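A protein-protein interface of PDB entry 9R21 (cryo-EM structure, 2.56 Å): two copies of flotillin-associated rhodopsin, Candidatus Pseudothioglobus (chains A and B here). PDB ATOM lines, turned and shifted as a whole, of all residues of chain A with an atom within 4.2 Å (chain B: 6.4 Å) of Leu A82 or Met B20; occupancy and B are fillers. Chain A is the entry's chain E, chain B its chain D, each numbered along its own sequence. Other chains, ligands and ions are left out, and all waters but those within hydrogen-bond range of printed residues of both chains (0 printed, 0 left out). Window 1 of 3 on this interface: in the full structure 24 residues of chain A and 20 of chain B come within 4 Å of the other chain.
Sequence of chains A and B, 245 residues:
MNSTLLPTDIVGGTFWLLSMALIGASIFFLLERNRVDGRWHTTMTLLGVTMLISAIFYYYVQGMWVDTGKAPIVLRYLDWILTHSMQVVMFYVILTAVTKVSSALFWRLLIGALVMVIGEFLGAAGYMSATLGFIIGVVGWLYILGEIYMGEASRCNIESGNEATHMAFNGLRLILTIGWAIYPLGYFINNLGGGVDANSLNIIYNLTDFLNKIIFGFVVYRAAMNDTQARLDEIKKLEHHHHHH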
ATOM      1  N   ILE A  53     -25.183  -0.042  29.659  1.00  0.00           N
ATOM      2  CA  ILE A  53     -24.719   1.133  28.946  1.00  0.00           C
ATOM      3  C   ILE A  53     -23.820   1.890  29.899  1.00  0.00           C
ATOM      4  O   ILE A  53     -22.727   2.319  29.565  1.00  0.00           O
ATOM      5  CB  ILE A  53     -25.917   1.943  28.431  1.00  0.00           C
ATOM      6  CG1 ILE A  53     -26.510   1.210  27.211  1.00  0.00           C
ATOM      7  CG2 ILE A  53     -25.555   3.394  28.101  1.00  0.00           C
ATOM      8  CD1 ILE A  53     -27.831   1.774  26.702  1.00  0.00           C
ATOM      9  N   ILE A  56     -20.433   0.412  30.312  1.00  0.00           N
ATOM     10  CA  ILE A  56     -19.585   0.630  29.154  1.00  0.00           C
ATOM     11  C   ILE A  56     -19.046   2.060  29.167  1.00  0.00           C
ATOM     12  O   ILE A  56     -17.895   2.272  28.855  1.00  0.00           O
ATOM     13  CB  ILE A  56     -20.378   0.305  27.890  1.00  0.00           C
ATOM     14  CG1 ILE A  56     -20.575  -1.179  27.832  1.00  0.00           C
ATOM     15  CG2 ILE A  56     -19.675   0.845  26.652  1.00  0.00           C
ATOM     16  CD1 ILE A  56     -21.594  -1.645  26.831  1.00  0.00           C
ATOM     17  N   PHE A  57     -19.855   3.011  29.576  1.00  0.00           N
ATOM     18  CA  PHE A  57     -19.342   4.318  29.859  1.00  0.00           C
ATOM     19  C   PHE A  57     -18.156   4.233  30.810  1.00  0.00           C
ATOM     20  O   PHE A  57     -17.085   4.743  30.512  1.00  0.00           O
ATOM     21  CB  PHE A  57     -20.513   5.147  30.395  1.00  0.00           C
ATOM     22  CG  PHE A  57     -20.096   6.531  30.842  1.00  0.00           C
ATOM     23  CD1 PHE A  57     -19.812   6.768  32.183  1.00  0.00           C
ATOM     24  CD2 PHE A  57     -19.849   7.543  29.909  1.00  0.00           C
ATOM     25  CE1 PHE A  57     -19.429   8.047  32.609  1.00  0.00           C
ATOM     26  CE2 PHE A  57     -19.417   8.806  30.328  1.00  0.00           C
ATOM     27  CZ  PHE A  57     -19.240   9.070  31.684  1.00  0.00           C
ATOM     28  N   LEU A  78     -22.714  12.024  27.927  1.00  0.00           N
ATOM     29  CA  LEU A  78     -22.826  10.873  27.063  1.00  0.00           C
ATOM     30  C   LEU A  78     -23.637   9.773  27.724  1.00  0.00           C
ATOM     31  O   LEU A  78     -24.406   9.097  27.040  1.00  0.00           O
ATOM     32  CB  LEU A  78     -21.427  10.329  26.785  1.00  0.00           C
ATOM     33  CG  LEU A  78     -20.518  11.263  25.992  1.00  0.00           C
ATOM     34  CD1 LEU A  78     -19.160  10.584  25.940  1.00  0.00           C
ATOM     35  CD2 LEU A  78     -21.114  11.552  24.616  1.00  0.00           C
ATOM     36  N   ASP A  79     -23.322   9.496  28.999  1.00  0.00           N
ATOM     37  CA  ASP A  79     -24.030   8.520  29.807  1.00  0.00           C
ATOM     38  C   ASP A  79     -25.462   9.024  29.999  1.00  0.00           C
ATOM     39  O   ASP A  79     -26.410   8.359  29.622  1.00  0.00           O
ATOM     40  CB  ASP A  79     -23.280   8.316  31.123  1.00  0.00           C
ATOM     41  CG  ASP A  79     -23.868   7.400  32.218  1.00  0.00           C
ATOM     42  OD1 ASP A  79     -24.707   6.507  31.916  1.00  0.00           O
ATOM     43  OD2 ASP A  79     -23.493   7.578  33.418  1.00  0.00           O
ATOM     44  N   TRP A  80     -25.619  10.213  30.560  1.00  0.00           N
ATOM     45  CA  TRP A  80     -26.926  10.723  30.909  1.00  0.00           C
ATOM     46  C   TRP A  80     -27.870  10.906  29.728  1.00  0.00           C
ATOM     47  O   TRP A  80     -29.077  10.783  29.890  1.00  0.00           O
ATOM     48  CB  TRP A  80     -26.787  12.064  31.631  1.00  0.00           C
ATOM     49  CG  TRP A  80     -25.963  11.964  32.876  1.00  0.00           C
ATOM     50  CD1 TRP A  80     -25.598  10.831  33.536  1.00  0.00           C
ATOM     51  CD2 TRP A  80     -25.348  13.054  33.581  1.00  0.00           C
ATOM     52  NE1 TRP A  80     -24.835  11.139  34.630  1.00  0.00           N
ATOM     53  CE2 TRP A  80     -24.651  12.489  34.680  1.00  0.00           C
ATOM     54  CE3 TRP A  80     -25.310  14.439  33.386  1.00  0.00           C
ATOM     55  CZ2 TRP A  80     -23.905  13.255  35.562  1.00  0.00           C
ATOM     56  CZ3 TRP A  80     -24.567  15.196  34.267  1.00  0.00           C
ATOM     57  CH2 TRP A  80     -23.859  14.607  35.317  1.00  0.00           C
ATOM     58  N   ILE A  81     -27.361  11.213  28.535  1.00  0.00           N
ATOM     59  CA  ILE A  81     -28.277  11.335  27.419  1.00  0.00           C
ATOM     60  C   ILE A  81     -28.981   9.991  27.200  1.00  0.00           C
ATOM     61  O   ILE A  81     -30.182   9.939  26.919  1.00  0.00           O
ATOM     62  CB  ILE A  81     -27.582  11.879  26.162  1.00  0.00           C
ATOM     63  CG1 ILE A  81     -28.587  12.337  25.139  1.00  0.00           C
ATOM     64  CG2 ILE A  81     -26.664  10.829  25.559  1.00  0.00           C
ATOM     65  CD1 ILE A  81     -29.655  13.289  25.662  1.00  0.00           C
ATOM     66  N   LEU A  82     -28.244   8.899  27.381  1.00  0.00           N
ATOM     67  CA  LEU A  82     -28.850   7.598  27.228  1.00  0.00           C
ATOM     68  C   LEU A  82     -29.551   7.142  28.498  1.00  0.00           C
ATOM     69  O   LEU A  82     -30.741   6.857  28.454  1.00  0.00           O
ATOM     70  CB  LEU A  82     -27.809   6.591  26.786  1.00  0.00           C
ATOM     71  CG  LEU A  82     -27.157   6.874  25.440  1.00  0.00           C
ATOM     72  CD1 LEU A  82     -26.203   5.714  25.125  1.00  0.00           C
ATOM     73  CD2 LEU A  82     -28.203   7.048  24.369  1.00  0.00           C
ATOM     74  N   THR A  83     -28.836   7.058  29.606  1.00  0.00           N
ATOM     75  CA  THR A  83     -29.358   6.375  30.779  1.00  0.00           C
ATOM     76  C   THR A  83     -30.372   7.245  31.549  1.00  0.00           C
ATOM     77  O   THR A  83     -31.229   6.701  32.227  1.00  0.00           O
ATOM     78  CB  THR A  83     -28.206   5.891  31.680  1.00  0.00           C
ATOM     79  OG1 THR A  83     -27.488   6.972  32.292  1.00  0.00           O
ATOM     80  CG2 THR A  83     -27.248   4.987  30.933  1.00  0.00           C
ATOM     81  N   HIS A  84     -30.334   8.569  31.484  1.00  0.00           N
ATOM     82  CA  HIS A  84     -31.367   9.287  32.213  1.00  0.00           C
ATOM     83  C   HIS A  84     -32.708   9.202  31.507  1.00  0.00           C
ATOM     84  O   HIS A  84     -33.742   9.329  32.156  1.00  0.00           O
ATOM     85  CB  HIS A  84     -31.053  10.761  32.454  1.00  0.00           C
ATOM     86  CG  HIS A  84     -30.055  10.937  33.532  1.00  0.00           C
ATOM     87  ND1 HIS A  84     -29.636  12.178  33.952  1.00  0.00           N
ATOM     88  CD2 HIS A  84     -29.372  10.011  34.254  1.00  0.00           C
ATOM     89  CE1 HIS A  84     -28.750  11.986  34.935  1.00  0.00           C
ATOM     90  NE2 HIS A  84     -28.561  10.685  35.127  1.00  0.00           N
ATOM     91  N   SER A  85     -32.651   9.024  30.190  1.00  0.00           N
ATOM     92  CA  SER A  85     -33.816   8.848  29.338  1.00  0.00           C
ATOM     93  C   SER A  85     -34.406   7.470  29.585  1.00  0.00           C
ATOM     94  O   SER A  85     -35.623   7.314  29.649  1.00  0.00           O
ATOM     95  CB  SER A  85     -33.450   8.992  27.885  1.00  0.00           C
ATOM     96  OG  SER A  85     -32.830  10.251  27.656  1.00  0.00           O
ATOM     97  N   MET A  86     -33.533   6.473  29.686  1.00  0.00           N
ATOM     98  CA  MET A  86     -33.995   5.131  29.956  1.00  0.00           C
ATOM     99  C   MET A  86     -34.615   5.060  31.345  1.00  0.00           C
ATOM    100  O   MET A  86     -35.681   4.468  31.513  1.00  0.00           O
ATOM    101  CB  MET A  86     -32.878   4.126  29.743  1.00  0.00           C
ATOM    102  CG  MET A  86     -32.524   4.051  28.264  1.00  0.00           C
ATOM    103  SD  MET A  86     -30.915   3.295  27.958  1.00  0.00           S
ATOM    104  CE  MET A  86     -31.386   1.568  28.143  1.00  0.00           C
ATOM    105  N   PHE B  15     -18.632   9.050  18.964  1.00  0.00           N
ATOM    106  CA  PHE B  15     -18.301   7.674  18.667  1.00  0.00           C
ATOM    107  C   PHE B  15     -18.622   6.820  19.894  1.00  0.00           C
ATOM    108  O   PHE B  15     -19.105   5.695  19.784  1.00  0.00           O
ATOM    109  CB  PHE B  15     -16.856   7.421  18.213  1.00  0.00           C
ATOM    110  CG  PHE B  15     -16.436   7.975  16.858  1.00  0.00           C
ATOM    111  CD1 PHE B  15     -17.251   7.896  15.741  1.00  0.00           C
ATOM    112  CD2 PHE B  15     -15.211   8.596  16.712  1.00  0.00           C
ATOM    113  CE1 PHE B  15     -16.870   8.432  14.520  1.00  0.00           C
ATOM    114  CE2 PHE B  15     -14.849   9.166  15.508  1.00  0.00           C
ATOM    115  CZ  PHE B  15     -15.681   9.075  14.412  1.00  0.00           C
ATOM    116  N   TRP B  16     -18.321   7.315  21.075  1.00  0.00           N
ATOM    117  CA  TRP B  16     -18.646   6.550  22.266  1.00  0.00           C
ATOM    118  C   TRP B  16     -20.160   6.439  22.453  1.00  0.00           C
ATOM    119  O   TRP B  16     -20.683   5.396  22.835  1.00  0.00           O
ATOM    120  CB  TRP B  16     -17.981   7.222  23.469  1.00  0.00           C
ATOM    121  CG  TRP B  16     -16.521   6.941  23.620  1.00  0.00           C
ATOM    122  CD1 TRP B  16     -15.702   6.123  22.894  1.00  0.00           C
ATOM    123  CD2 TRP B  16     -15.724   7.464  24.694  1.00  0.00           C
ATOM    124  NE1 TRP B  16     -14.434   6.136  23.411  1.00  0.00           N
ATOM    125  CE2 TRP B  16     -14.423   6.939  24.525  1.00  0.00           C
ATOM    126  CE3 TRP B  16     -16.001   8.298  25.786  1.00  0.00           C
ATOM    127  CZ2 TRP B  16     -13.395   7.250  25.408  1.00  0.00           C
ATOM    128  CZ3 TRP B  16     -14.991   8.561  26.682  1.00  0.00           C
ATOM    129  CH2 TRP B  16     -13.709   8.043  26.487  1.00  0.00           C
ATOM    130  N   LEU B  17     -20.851   7.551  22.226  1.00  0.00           N
ATOM    131  CA  LEU B  17     -22.286   7.577  22.373  1.00  0.00           C
ATOM    132  C   LEU B  17     -22.901   6.521  21.479  1.00  0.00           C
ATOM    133  O   LEU B  17     -23.670   5.689  21.965  1.00  0.00           O
ATOM    134  CB  LEU B  17     -22.767   8.963  22.029  1.00  0.00           C
ATOM    135  CG  LEU B  17     -24.268   9.175  22.127  1.00  0.00           C
ATOM    136  CD1 LEU B  17     -24.804   8.904  23.479  1.00  0.00           C
ATOM    137  CD2 LEU B  17     -24.497  10.616  21.747  1.00  0.00           C
ATOM    138  N   LEU B  18     -22.463   6.509  20.215  1.00  0.00           N
ATOM    139  CA  LEU B  18     -23.011   5.589  19.246  1.00  0.00           C
ATOM    140  C   LEU B  18     -22.733   4.161  19.654  1.00  0.00           C
ATOM    141  O   LEU B  18     -23.631   3.349  19.672  1.00  0.00           O
ATOM    142  CB  LEU B  18     -22.590   5.923  17.826  1.00  0.00           C
ATOM    143  CG  LEU B  18     -23.595   6.838  17.111  1.00  0.00           C
ATOM    144  CD1 LEU B  18     -24.903   6.131  16.835  1.00  0.00           C
ATOM    145  CD2 LEU B  18     -23.947   8.098  17.916  1.00  0.00           C
ATOM    146  N   SER B  19     -21.523   3.915  20.048  1.00  0.00           N
ATOM    147  CA  SER B  19     -21.080   2.613  20.481  1.00  0.00           C
ATOM    148  C   SER B  19     -21.997   2.077  21.581  1.00  0.00           C
ATOM    149  O   SER B  19     -22.456   0.924  21.508  1.00  0.00           O
ATOM    150  CB  SER B  19     -19.653   2.765  20.970  1.00  0.00           C
ATOM    151  OG  SER B  19     -19.026   1.497  20.896  1.00  0.00           O
ATOM    152  N   MET B  20     -22.247   2.921  22.597  1.00  0.00           N
ATOM    153  CA  MET B  20     -23.052   2.553  23.743  1.00  0.00           C
ATOM    154  C   MET B  20     -24.518   2.325  23.348  1.00  0.00           C
ATOM    155  O   MET B  20     -25.149   1.332  23.707  1.00  0.00           O
ATOM    156  CB  MET B  20     -22.969   3.647  24.809  1.00  0.00           C
ATOM    157  CG  MET B  20     -21.684   3.648  25.644  1.00  0.00           C
ATOM    158  SD  MET B  20     -21.263   5.306  26.258  1.00  0.00           S
ATOM    159  CE  MET B  20     -22.709   5.691  27.240  1.00  0.00           C
ATOM    160  N   ALA B  21     -25.086   3.282  22.630  1.00  0.00           N
ATOM    161  CA  ALA B  21     -26.472   3.180  22.243  1.00  0.00           C
ATOM    162  C   ALA B  21     -26.683   1.914  21.413  1.00  0.00           C
ATOM    163  O   ALA B  21     -27.692   1.224  21.557  1.00  0.00           O
ATOM    164  CB  ALA B  21     -26.873   4.430  21.505  1.00  0.00           C
ATOM    165  N   LEU B  22     -25.713   1.562  20.585  1.00  0.00           N
ATOM    166  CA  LEU B  22     -25.932   0.486  19.649  1.00  0.00           C
ATOM    167  C   LEU B  22     -25.777  -0.860  20.339  1.00  0.00           C
ATOM    168  O   LEU B  22     -26.568  -1.768  20.070  1.00  0.00           O
ATOM    169  CB  LEU B  22     -25.005   0.607  18.444  1.00  0.00           C
ATOM    170  CG  LEU B  22     -25.420   1.665  17.428  1.00  0.00           C
ATOM    171  CD1 LEU B  22     -24.226   2.015  16.524  1.00  0.00           C
ATOM    172  CD2 LEU B  22     -26.632   1.130  16.670  1.00  0.00           C
ATOM    173  N   ILE B  23     -24.784  -1.005  21.205  1.00  0.00           N
ATOM    174  CA  ILE B  23     -24.703  -2.245  21.972  1.00  0.00           C
ATOM    175  C   ILE B  23     -25.944  -2.414  22.853  1.00  0.00           C
ATOM    176  O   ILE B  23     -26.475  -3.516  22.983  1.00  0.00           O
ATOM    177  CB  ILE B  23     -23.392  -2.339  22.760  1.00  0.00           C
ATOM    178  CG1 ILE B  23     -23.216  -3.700  23.301  1.00  0.00           C
ATOM    179  CG2 ILE B  23     -23.316  -1.292  23.851  1.00  0.00           C
ATOM    180  CD1 ILE B  23     -23.199  -4.751  22.189  1.00  0.00           C
ATOM    181  N   GLY B  24     -26.490  -1.289  23.336  1.00  0.00           N
ATOM    182  CA  GLY B  24     -27.726  -1.293  24.093  1.00  0.00           C
ATOM    183  C   GLY B  24     -28.890  -1.816  23.287  1.00  0.00           C
ATOM    184  O   GLY B  24     -29.530  -2.794  23.664  1.00  0.00           O
ATOM    185  N   ALA B  25     -29.102  -1.187  22.143  1.00  0.00           N
ATOM    186  CA  ALA B  25     -30.172  -1.571  21.226  1.00  0.00           C
ATOM    187  C   ALA B  25     -30.064  -3.038  20.817  1.00  0.00           C
ATOM    188  O   ALA B  25     -31.041  -3.757  20.764  1.00  0.00           O
ATOM    189  CB  ALA B  25     -30.131  -0.652  20.047  1.00  0.00           C
ATOM    190  N   ALA B  55     -22.228  -1.543  16.153  1.00  0.00           N
ATOM    191  CA  ALA B  55     -21.566  -1.195  17.386  1.00  0.00           C
ATOM    192  C   ALA B  55     -20.093  -1.527  17.291  1.00  0.00           C
ATOM    193  O   ALA B  55     -19.270  -0.806  17.840  1.00  0.00           O
ATOM    194  CB  ALA B  55     -22.238  -1.931  18.537  1.00  0.00           C
ATOM    195  N   PHE B 210     -28.720   7.661  14.880  1.00  0.00           N
ATOM    196  CA  PHE B 210     -29.782   7.561  15.857  1.00  0.00           C
ATOM    197  C   PHE B 210     -31.095   7.296  15.134  1.00  0.00           C
ATOM    198  O   PHE B 210     -31.881   6.445  15.532  1.00  0.00           O
ATOM    199  CB  PHE B 210     -29.860   8.844  16.709  1.00  0.00           C
ATOM    200  CG  PHE B 210     -29.142   8.634  18.025  1.00  0.00           C
ATOM    201  CD1 PHE B 210     -29.687   7.789  18.995  1.00  0.00           C
ATOM    202  CD2 PHE B 210     -27.880   9.162  18.230  1.00  0.00           C
ATOM    203  CE1 PHE B 210     -28.982   7.493  20.153  1.00  0.00           C
ATOM    204  CE2 PHE B 210     -27.200   8.896  19.412  1.00  0.00           C
ATOM    205  CZ  PHE B 210     -27.748   8.058  20.365  1.00  0.00           C
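Of the 13 printed residues of chain B, 5 touch a printed residue of chain A.
Of the 12 printed residues of chain A, 6 touch a printed residue of chain B.
Printed residues of chain A that touch a printed residue of chain B: Ile A53, Ile A56, Phe A57, Leu A78, Ile A81 and Leu A82.
Hydrophobic or aromatic side chains of chain A that line the printed part of chain B: Ile A53, Ile A56, Phe A57, Leu A78, Ile A81 and Leu A82.
Among the printed residues, 11 pairs touch across the chains.
Among the printed residues, no Asp or Glu carboxylate lies within 4 Å of a Lys or Arg side-chain nitrogen of the other chain.
Leu A82 touches three residues of chain B.
Met B20 touches just these residues of chain A: Ile A53, Ile A56, Phe A57, Leu A78 and Leu A82.
Of the printed residues of chain A, Ile B23 touches Ile A56.
Of the printed residues of chain A, Ala B21 touches Leu A82.
Printed residues of chain A within 4 Å of Leu B17: Leu A78, Ile A81 and Leu A82.
Leu B22 touches none of the printed residues of chain A.
The nearest residue of chain A that does not touch Met B20 is Asp A79 (4.04 Å).
CE of Met B20 touches CG2 of Ile A53 (3.8 Å).
Ile A56 touches Met B20.
Ile A56 touches Ile B23.
Phe A57 touches Met B20 (CB to CE, 3.9 Å).
CE3 of Trp B16 touches CD1 of Leu A78 (3.9 Å).
Leu A78 touches Leu B17.
Leu A78 touches Met B20.
Leu B17 touches Ile A81 (CD1 to CG2, 3.4 Å).
CB of Met B20 touches CD1 of Leu A82, 3.9 Å away.
Ala B21 touches Leu A82 (N to CD1, 3.7 Å).
The backbone carbonyl oxygen (O) of Ile A81 sits at hydrogen-bond distance from the side-chain hydroxyl (OG) of Ser A85, 2.8 Å away.
No position is printed for both chains.
Of the 11 pairs that touch across the chains among the printed residues, none has its exchanged pair printed and touching as well.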
